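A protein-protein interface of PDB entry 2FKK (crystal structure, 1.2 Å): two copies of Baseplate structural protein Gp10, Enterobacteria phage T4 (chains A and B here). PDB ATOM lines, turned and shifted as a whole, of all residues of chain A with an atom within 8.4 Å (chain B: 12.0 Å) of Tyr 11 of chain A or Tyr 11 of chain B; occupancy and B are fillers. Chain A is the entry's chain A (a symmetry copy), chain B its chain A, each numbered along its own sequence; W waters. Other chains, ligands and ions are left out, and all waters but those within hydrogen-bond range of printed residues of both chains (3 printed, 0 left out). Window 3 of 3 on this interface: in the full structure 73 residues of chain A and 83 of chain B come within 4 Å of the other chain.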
ATOM      1  N   LEU A  10     -24.503  20.101  20.675  1.00  0.00           N
ATOM      2  CA  LEU A  10     -24.912  19.849  22.016  1.00  0.00           C
ATOM      3  C   LEU A  10     -25.552  18.423  22.076  1.00  0.00           C
ATOM      4  O   LEU A  10     -25.703  17.796  21.042  1.00  0.00           O
ATOM      5  CB  LEU A  10     -25.923  20.770  22.654  1.00  0.00           C
ATOM      6  CG  LEU A  10     -26.499  22.116  22.569  1.00  0.00           C
ATOM      7  CD1 LEU A  10     -27.419  22.297  21.350  1.00  0.00           C
ATOM      8  CD2 LEU A  10     -27.297  22.388  23.865  1.00  0.00           C
ATOM      9  N   TYR A  11     -25.825  17.996  23.288  1.00  0.00           N
ATOM     10  CA  TYR A  11     -26.188  16.628  23.578  1.00  0.00           C
ATOM     11  C   TYR A  11     -27.587  16.524  24.145  1.00  0.00           C
ATOM     12  O   TYR A  11     -28.105  17.462  24.759  1.00  0.00           O
ATOM     13  CB  TYR A  11     -25.229  15.963  24.582  1.00  0.00           C
ATOM     14  CG  TYR A  11     -23.831  16.071  24.097  1.00  0.00           C
ATOM     15  CD1 TYR A  11     -23.450  15.533  22.889  1.00  0.00           C
ATOM     16  CD2 TYR A  11     -22.890  16.727  24.864  1.00  0.00           C
ATOM     17  CE1 TYR A  11     -22.162  15.619  22.392  1.00  0.00           C
ATOM     18  CE2 TYR A  11     -21.604  16.813  24.372  1.00  0.00           C
ATOM     19  CZ  TYR A  11     -21.247  16.270  23.161  1.00  0.00           C
ATOM     20  OH  TYR A  11     -19.944  16.372  22.720  1.00  0.00           O
ATOM     21  N   VAL A  12     -28.209  15.351  23.932  1.00  0.00           N
ATOM     22  CA  VAL A  12     -29.564  15.110  24.431  1.00  0.00           C
ATOM     23  C   VAL A  12     -29.506  14.890  25.930  1.00  0.00           C
ATOM     24  O   VAL A  12     -28.763  13.958  26.376  1.00  0.00           O
ATOM     25  CB  VAL A  12     -30.201  13.899  23.726  1.00  0.00           C
ATOM     26  CG1 VAL A  12     -31.599  13.643  24.291  1.00  0.00           C
ATOM     27  CG2 VAL A  12     -30.257  14.073  22.229  1.00  0.00           C
ATOM     28  N   SER A  13     -30.235  15.662  26.710  1.00  0.00           N
ATOM     29  CA  SER A  13     -30.336  15.438  28.140  1.00  0.00           C
ATOM     30  C   SER A  13     -31.122  14.190  28.468  1.00  0.00           C
ATOM     31  O   SER A  13     -32.148  13.906  27.799  1.00  0.00           O
ATOM     32  CB  SER A  13     -31.047  16.683  28.674  1.00  0.00           C
ATOM     33  OG  SER A  13     -31.451  16.724  30.002  1.00  0.00           O
ATOM     34  N   GLN A  14     -30.716  13.471  29.508  1.00  0.00           N
ATOM     35  CA  GLN A  14     -31.501  12.349  30.017  1.00  0.00           C
ATOM     36  C   GLN A  14     -32.858  12.761  30.503  1.00  0.00           C
ATOM     37  O   GLN A  14     -33.856  12.043  30.475  1.00  0.00           O
ATOM     38  CB  GLN A  14     -30.732  11.630  31.124  1.00  0.00           C
ATOM     39  CG  GLN A  14     -29.407  11.094  30.695  1.00  0.00           C
ATOM     40  CD  GLN A  14     -28.817  10.168  31.724  1.00  0.00           C
ATOM     41  OE1 GLN A  14     -29.441   9.760  32.681  1.00  0.00           O
ATOM     42  NE2 GLN A  14     -27.537   9.849  31.582  1.00  0.00           N
ATOM     43  N   GLY A  15     -32.987  13.949  31.007  1.00  0.00           N
ATOM     44  CA  GLY A  15     -34.248  14.495  31.546  1.00  0.00           C
ATOM     45  C   GLY A  15     -34.485  13.874  32.894  1.00  0.00           C
ATOM     46  O   GLY A  15     -33.637  13.107  33.349  1.00  0.00           O
ATOM     47  N   PHE A  47     -32.791   7.569  31.505  1.00  0.00           N
ATOM     48  CA  PHE A  47     -32.380   7.416  30.103  1.00  0.00           C
ATOM     49  C   PHE A  47     -30.856   7.507  29.986  1.00  0.00           C
ATOM     50  O   PHE A  47     -30.336   8.395  29.338  1.00  0.00           O
ATOM     51  CB  PHE A  47     -33.126   8.446  29.269  1.00  0.00           C
ATOM     52  CG  PHE A  47     -34.621   8.161  29.301  1.00  0.00           C
ATOM     53  CD1 PHE A  47     -35.165   7.080  28.635  1.00  0.00           C
ATOM     54  CD2 PHE A  47     -35.441   8.957  30.044  1.00  0.00           C
ATOM     55  CE1 PHE A  47     -36.486   6.774  28.744  1.00  0.00           C
ATOM     56  CE2 PHE A  47     -36.805   8.643  30.143  1.00  0.00           C
ATOM     57  CZ  PHE A  47     -37.335   7.550  29.495  1.00  0.00           C
ATOM     58  N   ASN A  48     -30.206   6.516  30.598  1.00  0.00           N
ATOM     59  CA  ASN A  48     -28.759   6.468  30.555  1.00  0.00           C
ATOM     60  C   ASN A  48     -28.177   6.261  29.159  1.00  0.00           C
ATOM     61  O   ASN A  48     -27.110   6.802  28.882  1.00  0.00           O
ATOM     62  CB  ASN A  48     -28.234   5.325  31.430  1.00  0.00           C
ATOM     63  CG  ASN A  48     -28.498   5.534  32.908  1.00  0.00           C
ATOM     64  OD1 ASN A  48     -28.577   6.659  33.377  1.00  0.00           O
ATOM     65  ND2 ASN A  48     -28.657   4.456  33.611  1.00  0.00           N
ATOM     66  N   ALA A  49     -28.887   5.499  28.360  1.00  0.00           N
ATOM     67  CA  ALA A  49     -28.379   5.146  27.032  1.00  0.00           C
ATOM     68  C   ALA A  49     -29.561   4.941  26.099  1.00  0.00           C
ATOM     69  O   ALA A  49     -30.736   4.896  26.500  1.00  0.00           O
ATOM     70  CB  ALA A  49     -27.527   3.916  27.067  1.00  0.00           C
ATOM     71  N   VAL A  50     -29.215   4.778  24.811  1.00  0.00           N
ATOM     72  CA  VAL A  50     -30.253   4.551  23.807  1.00  0.00           C
ATOM     73  C   VAL A  50     -31.138   3.375  24.124  1.00  0.00           C
ATOM     74  O   VAL A  50     -32.353   3.433  23.898  1.00  0.00           O
ATOM     75  CB  VAL A  50     -29.568   4.442  22.432  1.00  0.00           C
ATOM     76  CG1 VAL A  50     -30.606   4.037  21.389  1.00  0.00           C
ATOM     77  CG2 VAL A  50     -28.951   5.755  22.029  1.00  0.00           C
ATOM     78  N   ILE A  53     -34.155   4.486  26.026  1.00  0.00           N
ATOM     79  CA  ILE A  53     -35.118   5.144  25.146  1.00  0.00           C
ATOM     80  C   ILE A  53     -35.930   4.107  24.382  1.00  0.00           C
ATOM     81  O   ILE A  53     -37.163   4.190  24.294  1.00  0.00           O
ATOM     82  CB  ILE A  53     -34.442   6.129  24.218  1.00  0.00           C
ATOM     83  CG1 ILE A  53     -33.709   7.255  25.012  1.00  0.00           C
ATOM     84  CG2 ILE A  53     -35.453   6.756  23.251  1.00  0.00           C
ATOM     85  CD1 ILE A  53     -32.901   8.201  24.151  1.00  0.00           C
ATOM     86  N   LEU B  10     -27.502  15.401  33.054  1.00  0.00           N
ATOM     87  CA  LEU B  10     -26.610  14.500  32.403  1.00  0.00           C
ATOM     88  C   LEU B  10     -27.199  14.154  30.995  1.00  0.00           C
ATOM     89  O   LEU B  10     -28.302  14.577  30.694  1.00  0.00           O
ATOM     90  CB  LEU B  10     -26.315  13.171  33.052  1.00  0.00           C
ATOM     91  CG  LEU B  10     -26.332  12.467  34.338  1.00  0.00           C
ATOM     92  CD1 LEU B  10     -27.755  12.150  34.830  1.00  0.00           C
ATOM     93  CD2 LEU B  10     -25.532  11.152  34.185  1.00  0.00           C
ATOM     94  N   TYR B  11     -26.396  13.461  30.222  1.00  0.00           N
ATOM     95  CA  TYR B  11     -26.647  13.249  28.814  1.00  0.00           C
ATOM     96  C   TYR B  11     -26.839  11.784  28.490  1.00  0.00           C
ATOM     97  O   TYR B  11     -26.331  10.898  29.184  1.00  0.00           O
ATOM     98  CB  TYR B  11     -25.504  13.776  27.926  1.00  0.00           C
ATOM     99  CG  TYR B  11     -25.242  15.204  28.230  1.00  0.00           C
ATOM    100  CD1 TYR B  11     -26.224  16.158  28.087  1.00  0.00           C
ATOM    101  CD2 TYR B  11     -23.994  15.591  28.674  1.00  0.00           C
ATOM    102  CE1 TYR B  11     -26.027  17.499  28.369  1.00  0.00           C
ATOM    103  CE2 TYR B  11     -23.793  16.927  28.954  1.00  0.00           C
ATOM    104  CZ  TYR B  11     -24.790  17.861  28.805  1.00  0.00           C
ATOM    105  OH  TYR B  11     -24.536  19.187  29.087  1.00  0.00           O
ATOM    106  N   VAL B  12     -27.591  11.529  27.405  1.00  0.00           N
ATOM    107  CA  VAL B  12     -27.854  10.155  26.972  1.00  0.00           C
ATOM    108  C   VAL B  12     -26.603   9.594  26.325  1.00  0.00           C
ATOM    109  O   VAL B  12     -26.101  10.218  25.335  1.00  0.00           O
ATOM    110  CB  VAL B  12     -29.042  10.107  25.993  1.00  0.00           C
ATOM    111  CG1 VAL B  12     -29.272   8.670  25.524  1.00  0.00           C
ATOM    112  CG2 VAL B  12     -30.302  10.677  26.596  1.00  0.00           C
ATOM    113  N   SER B  13     -26.092   8.478  26.803  1.00  0.00           N
ATOM    114  CA  SER B  13     -24.974   7.807  26.166  1.00  0.00           C
ATOM    115  C   SER B  13     -25.360   7.184  24.844  1.00  0.00           C
ATOM    116  O   SER B  13     -26.475   6.616  24.725  1.00  0.00           O
ATOM    117  CB  SER B  13     -24.550   6.731  27.169  1.00  0.00           C
ATOM    118  OG  SER B  13     -23.596   5.791  26.801  1.00  0.00           O
ATOM    119  N   GLN B  14     -24.458   7.216  23.870  1.00  0.00           N
ATOM    120  CA  GLN B  14     -24.659   6.494  22.616  1.00  0.00           C
ATOM    121  C   GLN B  14     -24.776   5.012  22.810  1.00  0.00           C
ATOM    122  O   GLN B  14     -25.437   4.265  22.090  1.00  0.00           O
ATOM    123  CB  GLN B  14     -23.531   6.817  21.639  1.00  0.00           C
ATOM    124  CG  GLN B  14     -23.409   8.268  21.308  1.00  0.00           C
ATOM    125  CD  GLN B  14     -22.480   8.503  20.147  1.00  0.00           C
ATOM    126  OE1 GLN B  14     -22.053   7.605  19.451  1.00  0.00           O
ATOM    127  NE2 GLN B  14     -22.083   9.752  19.939  1.00  0.00           N
ATOM    128  N   GLY B  15     -24.122   4.476  23.792  1.00  0.00           N
ATOM    129  CA  GLY B  15     -24.117   3.031  24.102  1.00  0.00           C
ATOM    130  C   GLY B  15     -23.228   2.344  23.105  1.00  0.00           C
ATOM    131  O   GLY B  15     -22.630   3.029  22.274  1.00  0.00           O
ATOM    132  N   PRO B  16     -23.191   1.034  23.232  1.00  0.00           N
ATOM    133  CA  PRO B  16     -22.430   0.287  22.274  1.00  0.00           C
ATOM    134  C   PRO B  16     -23.336   0.371  21.023  1.00  0.00           C
ATOM    135  O   PRO B  16     -24.573   0.360  20.877  1.00  0.00           O
ATOM    136  CB  PRO B  16     -22.381  -1.105  22.780  1.00  0.00           C
ATOM    137  CG  PRO B  16     -23.337  -1.212  23.883  1.00  0.00           C
ATOM    138  CD  PRO B  16     -23.838   0.160  24.176  1.00  0.00           C
ATOM    139  N   PHE B  47     -25.140   5.532  17.559  1.00  0.00           N
ATOM    140  CA  PHE B  47     -26.180   6.530  17.842  1.00  0.00           C
ATOM    141  C   PHE B  47     -25.548   7.913  18.028  1.00  0.00           C
ATOM    142  O   PHE B  47     -25.645   8.500  19.088  1.00  0.00           O
ATOM    143  CB  PHE B  47     -26.990   6.054  19.038  1.00  0.00           C
ATOM    144  CG  PHE B  47     -27.725   4.767  18.693  1.00  0.00           C
ATOM    145  CD1 PHE B  47     -28.806   4.762  17.832  1.00  0.00           C
ATOM    146  CD2 PHE B  47     -27.283   3.582  19.200  1.00  0.00           C
ATOM    147  CE1 PHE B  47     -29.402   3.599  17.452  1.00  0.00           C
ATOM    148  CE2 PHE B  47     -27.908   2.387  18.814  1.00  0.00           C
ATOM    149  CZ  PHE B  47     -28.970   2.388  17.937  1.00  0.00           C
ATOM    150  N   ASN B  48     -24.964   8.392  16.930  1.00  0.00           N
ATOM    151  CA  ASN B  48     -24.339   9.699  16.958  1.00  0.00           C
ATOM    152  C   ASN B  48     -25.307  10.854  17.193  1.00  0.00           C
ATOM    153  O   ASN B  48     -24.917  11.824  17.836  1.00  0.00           O
ATOM    154  CB  ASN B  48     -23.624   9.980  15.632  1.00  0.00           C
ATOM    155  CG  ASN B  48     -22.437   9.069  15.388  1.00  0.00           C
ATOM    156  OD1 ASN B  48     -21.804   8.602  16.323  1.00  0.00           O
ATOM    157  ND2 ASN B  48     -22.170   8.809  14.145  1.00  0.00           N
ATOM    158  N   ALA B  49     -26.501  10.705  16.669  1.00  0.00           N
ATOM    159  CA  ALA B  49     -27.482  11.791  16.742  1.00  0.00           C
ATOM    160  C   ALA B  49     -28.876  11.186  16.768  1.00  0.00           C
ATOM    161  O   ALA B  49     -29.091   9.980  16.559  1.00  0.00           O
ATOM    162  CB  ALA B  49     -27.351  12.741  15.593  1.00  0.00           C
ATOM    163  N   VAL B  50     -29.851  12.079  17.005  1.00  0.00           N
ATOM    164  CA  VAL B  50     -31.244  11.636  17.038  1.00  0.00           C
ATOM    165  C   VAL B  50     -31.668  10.918  15.783  1.00  0.00           C
ATOM    166  O   VAL B  50     -32.412   9.933  15.854  1.00  0.00           O
ATOM    167  CB  VAL B  50     -32.123  12.858  17.366  1.00  0.00           C
ATOM    168  CG1 VAL B  50     -33.591  12.462  17.239  1.00  0.00           C
ATOM    169  CG2 VAL B  50     -31.864  13.352  18.764  1.00  0.00           C
ATOM    170  N   SER B  51     -31.181  11.333  14.610  1.00  0.00           N
ATOM    171  CA  SER B  51     -31.554  10.647  13.375  1.00  0.00           C
ATOM    172  C   SER B  51     -31.268   9.152  13.426  1.00  0.00           C
ATOM    173  O   SER B  51     -31.992   8.322  12.897  1.00  0.00           O
ATOM    174  CB  SER B  51     -30.744  11.259  12.233  1.00  0.00           C
ATOM    175  OG  SER B  51     -31.143  10.729  10.981  1.00  0.00           O
ATOM    176  N   ASN B  52     -30.134   8.764  14.035  1.00  0.00           N
ATOM    177  CA  ASN B  52     -29.786   7.362  14.161  1.00  0.00           C
ATOM    178  C   ASN B  52     -30.742   6.599  15.085  1.00  0.00           C
ATOM    179  O   ASN B  52     -31.062   5.439  14.819  1.00  0.00           O
ATOM    180  CB  ASN B  52     -28.341   7.192  14.706  1.00  0.00           C
ATOM    181  CG  ASN B  52     -27.309   7.943  13.866  1.00  0.00           C
ATOM    182  OD1 ASN B  52     -26.749   8.946  14.325  1.00  0.00           O
ATOM    183  ND2 ASN B  52     -27.105   7.420  12.660  1.00  0.00           N
ATOM    184  N   ILE B  53     -31.183   7.234  16.161  1.00  0.00           N
ATOM    185  CA  ILE B  53     -32.223   6.651  17.005  1.00  0.00           C
ATOM    186  C   ILE B  53     -33.501   6.443  16.204  1.00  0.00           C
ATOM    187  O   ILE B  53     -34.129   5.377  16.257  1.00  0.00           O
ATOM    188  CB  ILE B  53     -32.463   7.482  18.246  1.00  0.00           C
ATOM    189  CG1 ILE B  53     -31.174   7.592  19.120  1.00  0.00           C
ATOM    190  CG2 ILE B  53     -33.605   6.898  19.086  1.00  0.00           C
ATOM    191  CD1 ILE B  53     -31.305   8.515  20.311  1.00  0.00           C
HETATM  192  O   HOH W   1     -25.106   8.074  30.458  1.00  0.00           O
HETATM  193  O   HOH W   2     -30.604  15.393  32.535  1.00  0.00           O
HETATM  194  O   HOH W   3     -29.110  17.226  31.393  1.00  0.00           O
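The side-chain hydroxyl of Ser 13 of chain B lies close to the backbone NH of Gly 15 of chain B, 3.3 Å away. OE1 of Gln 14 of chain B lies close to OD1 of Asn 48 of chain B, 3.3 Å away. The side-chain hydroxyl (OG) of Ser 13 of chain A lies close to the backbone NH (N) of Gly 15 of chain A, 3.3 Å away. The side-chain amide oxygen (OE1) of Gln 14 of chain A lies close to the side-chain amide oxygen (OD1) of Asn 48 of chain A, 3.3 Å away.
Tyr 11 of chain A touches one residue of chain B. No residue of chain B comes within 4 Å of Leu 10 of chain A. Of chain B, only Leu 10, Tyr 11 and Val 12 come within 4 Å of Gln 14 of chain A. Of the printed residues of chain A, Leu 10 of chain B touches Ser 13 and Gln 14. Printed residues of chain A within 4 Å of Val 50 of chain B: Val 12 (3.9 Å). Printed residues of chain B within 4 Å of Phe 47 of chain A: Val 12. Asn 52 of chain B touches none of the printed residues of chain A. Pro 16 of chain B touches none of the printed residues of chain A. The nearest residue of chain B that does not touch Tyr 11 of chain A is Val 12 of chain B (5.8 Å). The nearest printed residue of chain A that does not touch Tyr 11 of chain B is Ser 13 of chain A (4.2 Å). The nearest printed residue of chain B that does not touch Asn 48 of chain A is Tyr 11 of chain B (4.2 Å).
N of Gln 14 of chain A sits at hydrogen-bond distance from O of Leu 10 of chain B, at 2.9 Å. The backbone carbonyl oxygen (O) of Tyr 11 of chain B sits at hydrogen-bond distance from the side-chain amide nitrogen (NE2) of Gln 14 of chain A, at 2.9 Å. The backbone NH (N) of Val 12 of chain B sits at hydrogen-bond distance from the backbone carbonyl oxygen (O) of Val 12 of chain A, 2.9 Å away. N of Ser 13 of chain B sits at hydrogen-bond distance from O of Asn 48 of chain A. The backbone NH of Val 50 of chain A lies within hydrogen-bond range of the backbone carbonyl oxygen of Ser 13 of chain B, at 3.3 Å.
Tyr 11 of chain B touches its own counterpart, Tyr 11 of chain A. Val 12 of chain A touches Val 50 of chain B, and with the chains exchanged Val 50 of chain A touches Val 12 of chain B. Ser 13 of chain A touches Val 12 of chain B, but with the chains exchanged Val 12 of chain A does not touch Ser 13 of chain B (6.1 Å). Gln 14 of chain A touches Leu 10 of chain B, but with the chains exchanged Leu 10 of chain A does not touch Gln 14 of chain B (8.9 Å). Positions printed for both chains: 10, 11, 12, 13, 14, 15, 47, 48, 49, 50 and 53.
Among the printed residues, merely in contact across the chains: Val 12 of chain A with Tyr 11 of chain B (3.3 Å), Ala 49 of chain A with Ser 13 of chain B (3.3 Å), Ser 13 of chain A with Leu 10 of chain B (3.4 Å), Phe 47 of chain A with Val 12 of chain B (3.6 Å), Val 50 of chain A with Phe 47 of chain B (3.6 Å), Tyr 11 of chain A with Tyr 11 of chain B (3.6 Å), Gln 14 of chain A with Val 12 of chain B (3.8 Å), Ala 49 of chain A with Val 12 of chain B (3.8 Å), Val 50 of chain A with Gln 14 of chain B (3.8 Å), Asn 48 of chain A with Val 12 of chain B (3.8 Å), Val 12 of chain A with Val 50 of chain B (3.9 Å), Ile 53 of chain A with Val 12 of chain B (3.9 Å), Ser 13 of chain A with Val 12 of chain B (3.9 Å) and Val 50 of chain A with Val 12 of chain B (3.96 Å).
Water W3 lies within hydrogen-bond range of OG of Ser 13 of chain A (2.8 Å) and O of Leu 10 of chain B (2.9 Å). Water W1 lies within hydrogen-bond range of the backbone carbonyl oxygen of Asn 48 of chain A (2.8 Å), the side-chain amide nitrogen of Gln 14 of chain A (3.2 Å) and the backbone carbonyl oxygen of Tyr 11 of chain B (3.3 Å). Water W2 lies within hydrogen-bond range of the side-chain hydroxyl of Ser 13 of chain A, the backbone carbonyl oxygen of Leu 10 of chain B and the backbone NH of Gly 15 of chain A.
Of the 11 printed residues of chain A, 9 touch a printed residue of chain B. Hydrophobic or aromatic side chains of chain A that line the printed part of chain B: Tyr 11, Val 12, Ala 49, Val 50 and Ile 53. Printed residues of chain B that touch a printed residue of chain A: Leu 10, Tyr 11, Val 12, Ser 13, Gln 14, Phe 47 and Val 50. Hydrophobic or aromatic side chains of chain B within 4 Å of the printed part of chain A: Leu 10, Tyr 11, Val 12, Phe 47 and Val 50. Among the printed residues, no Asp or Glu carboxylate lies within 4 Å of a Lys or Arg side-chain nitrogen of the other chain.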
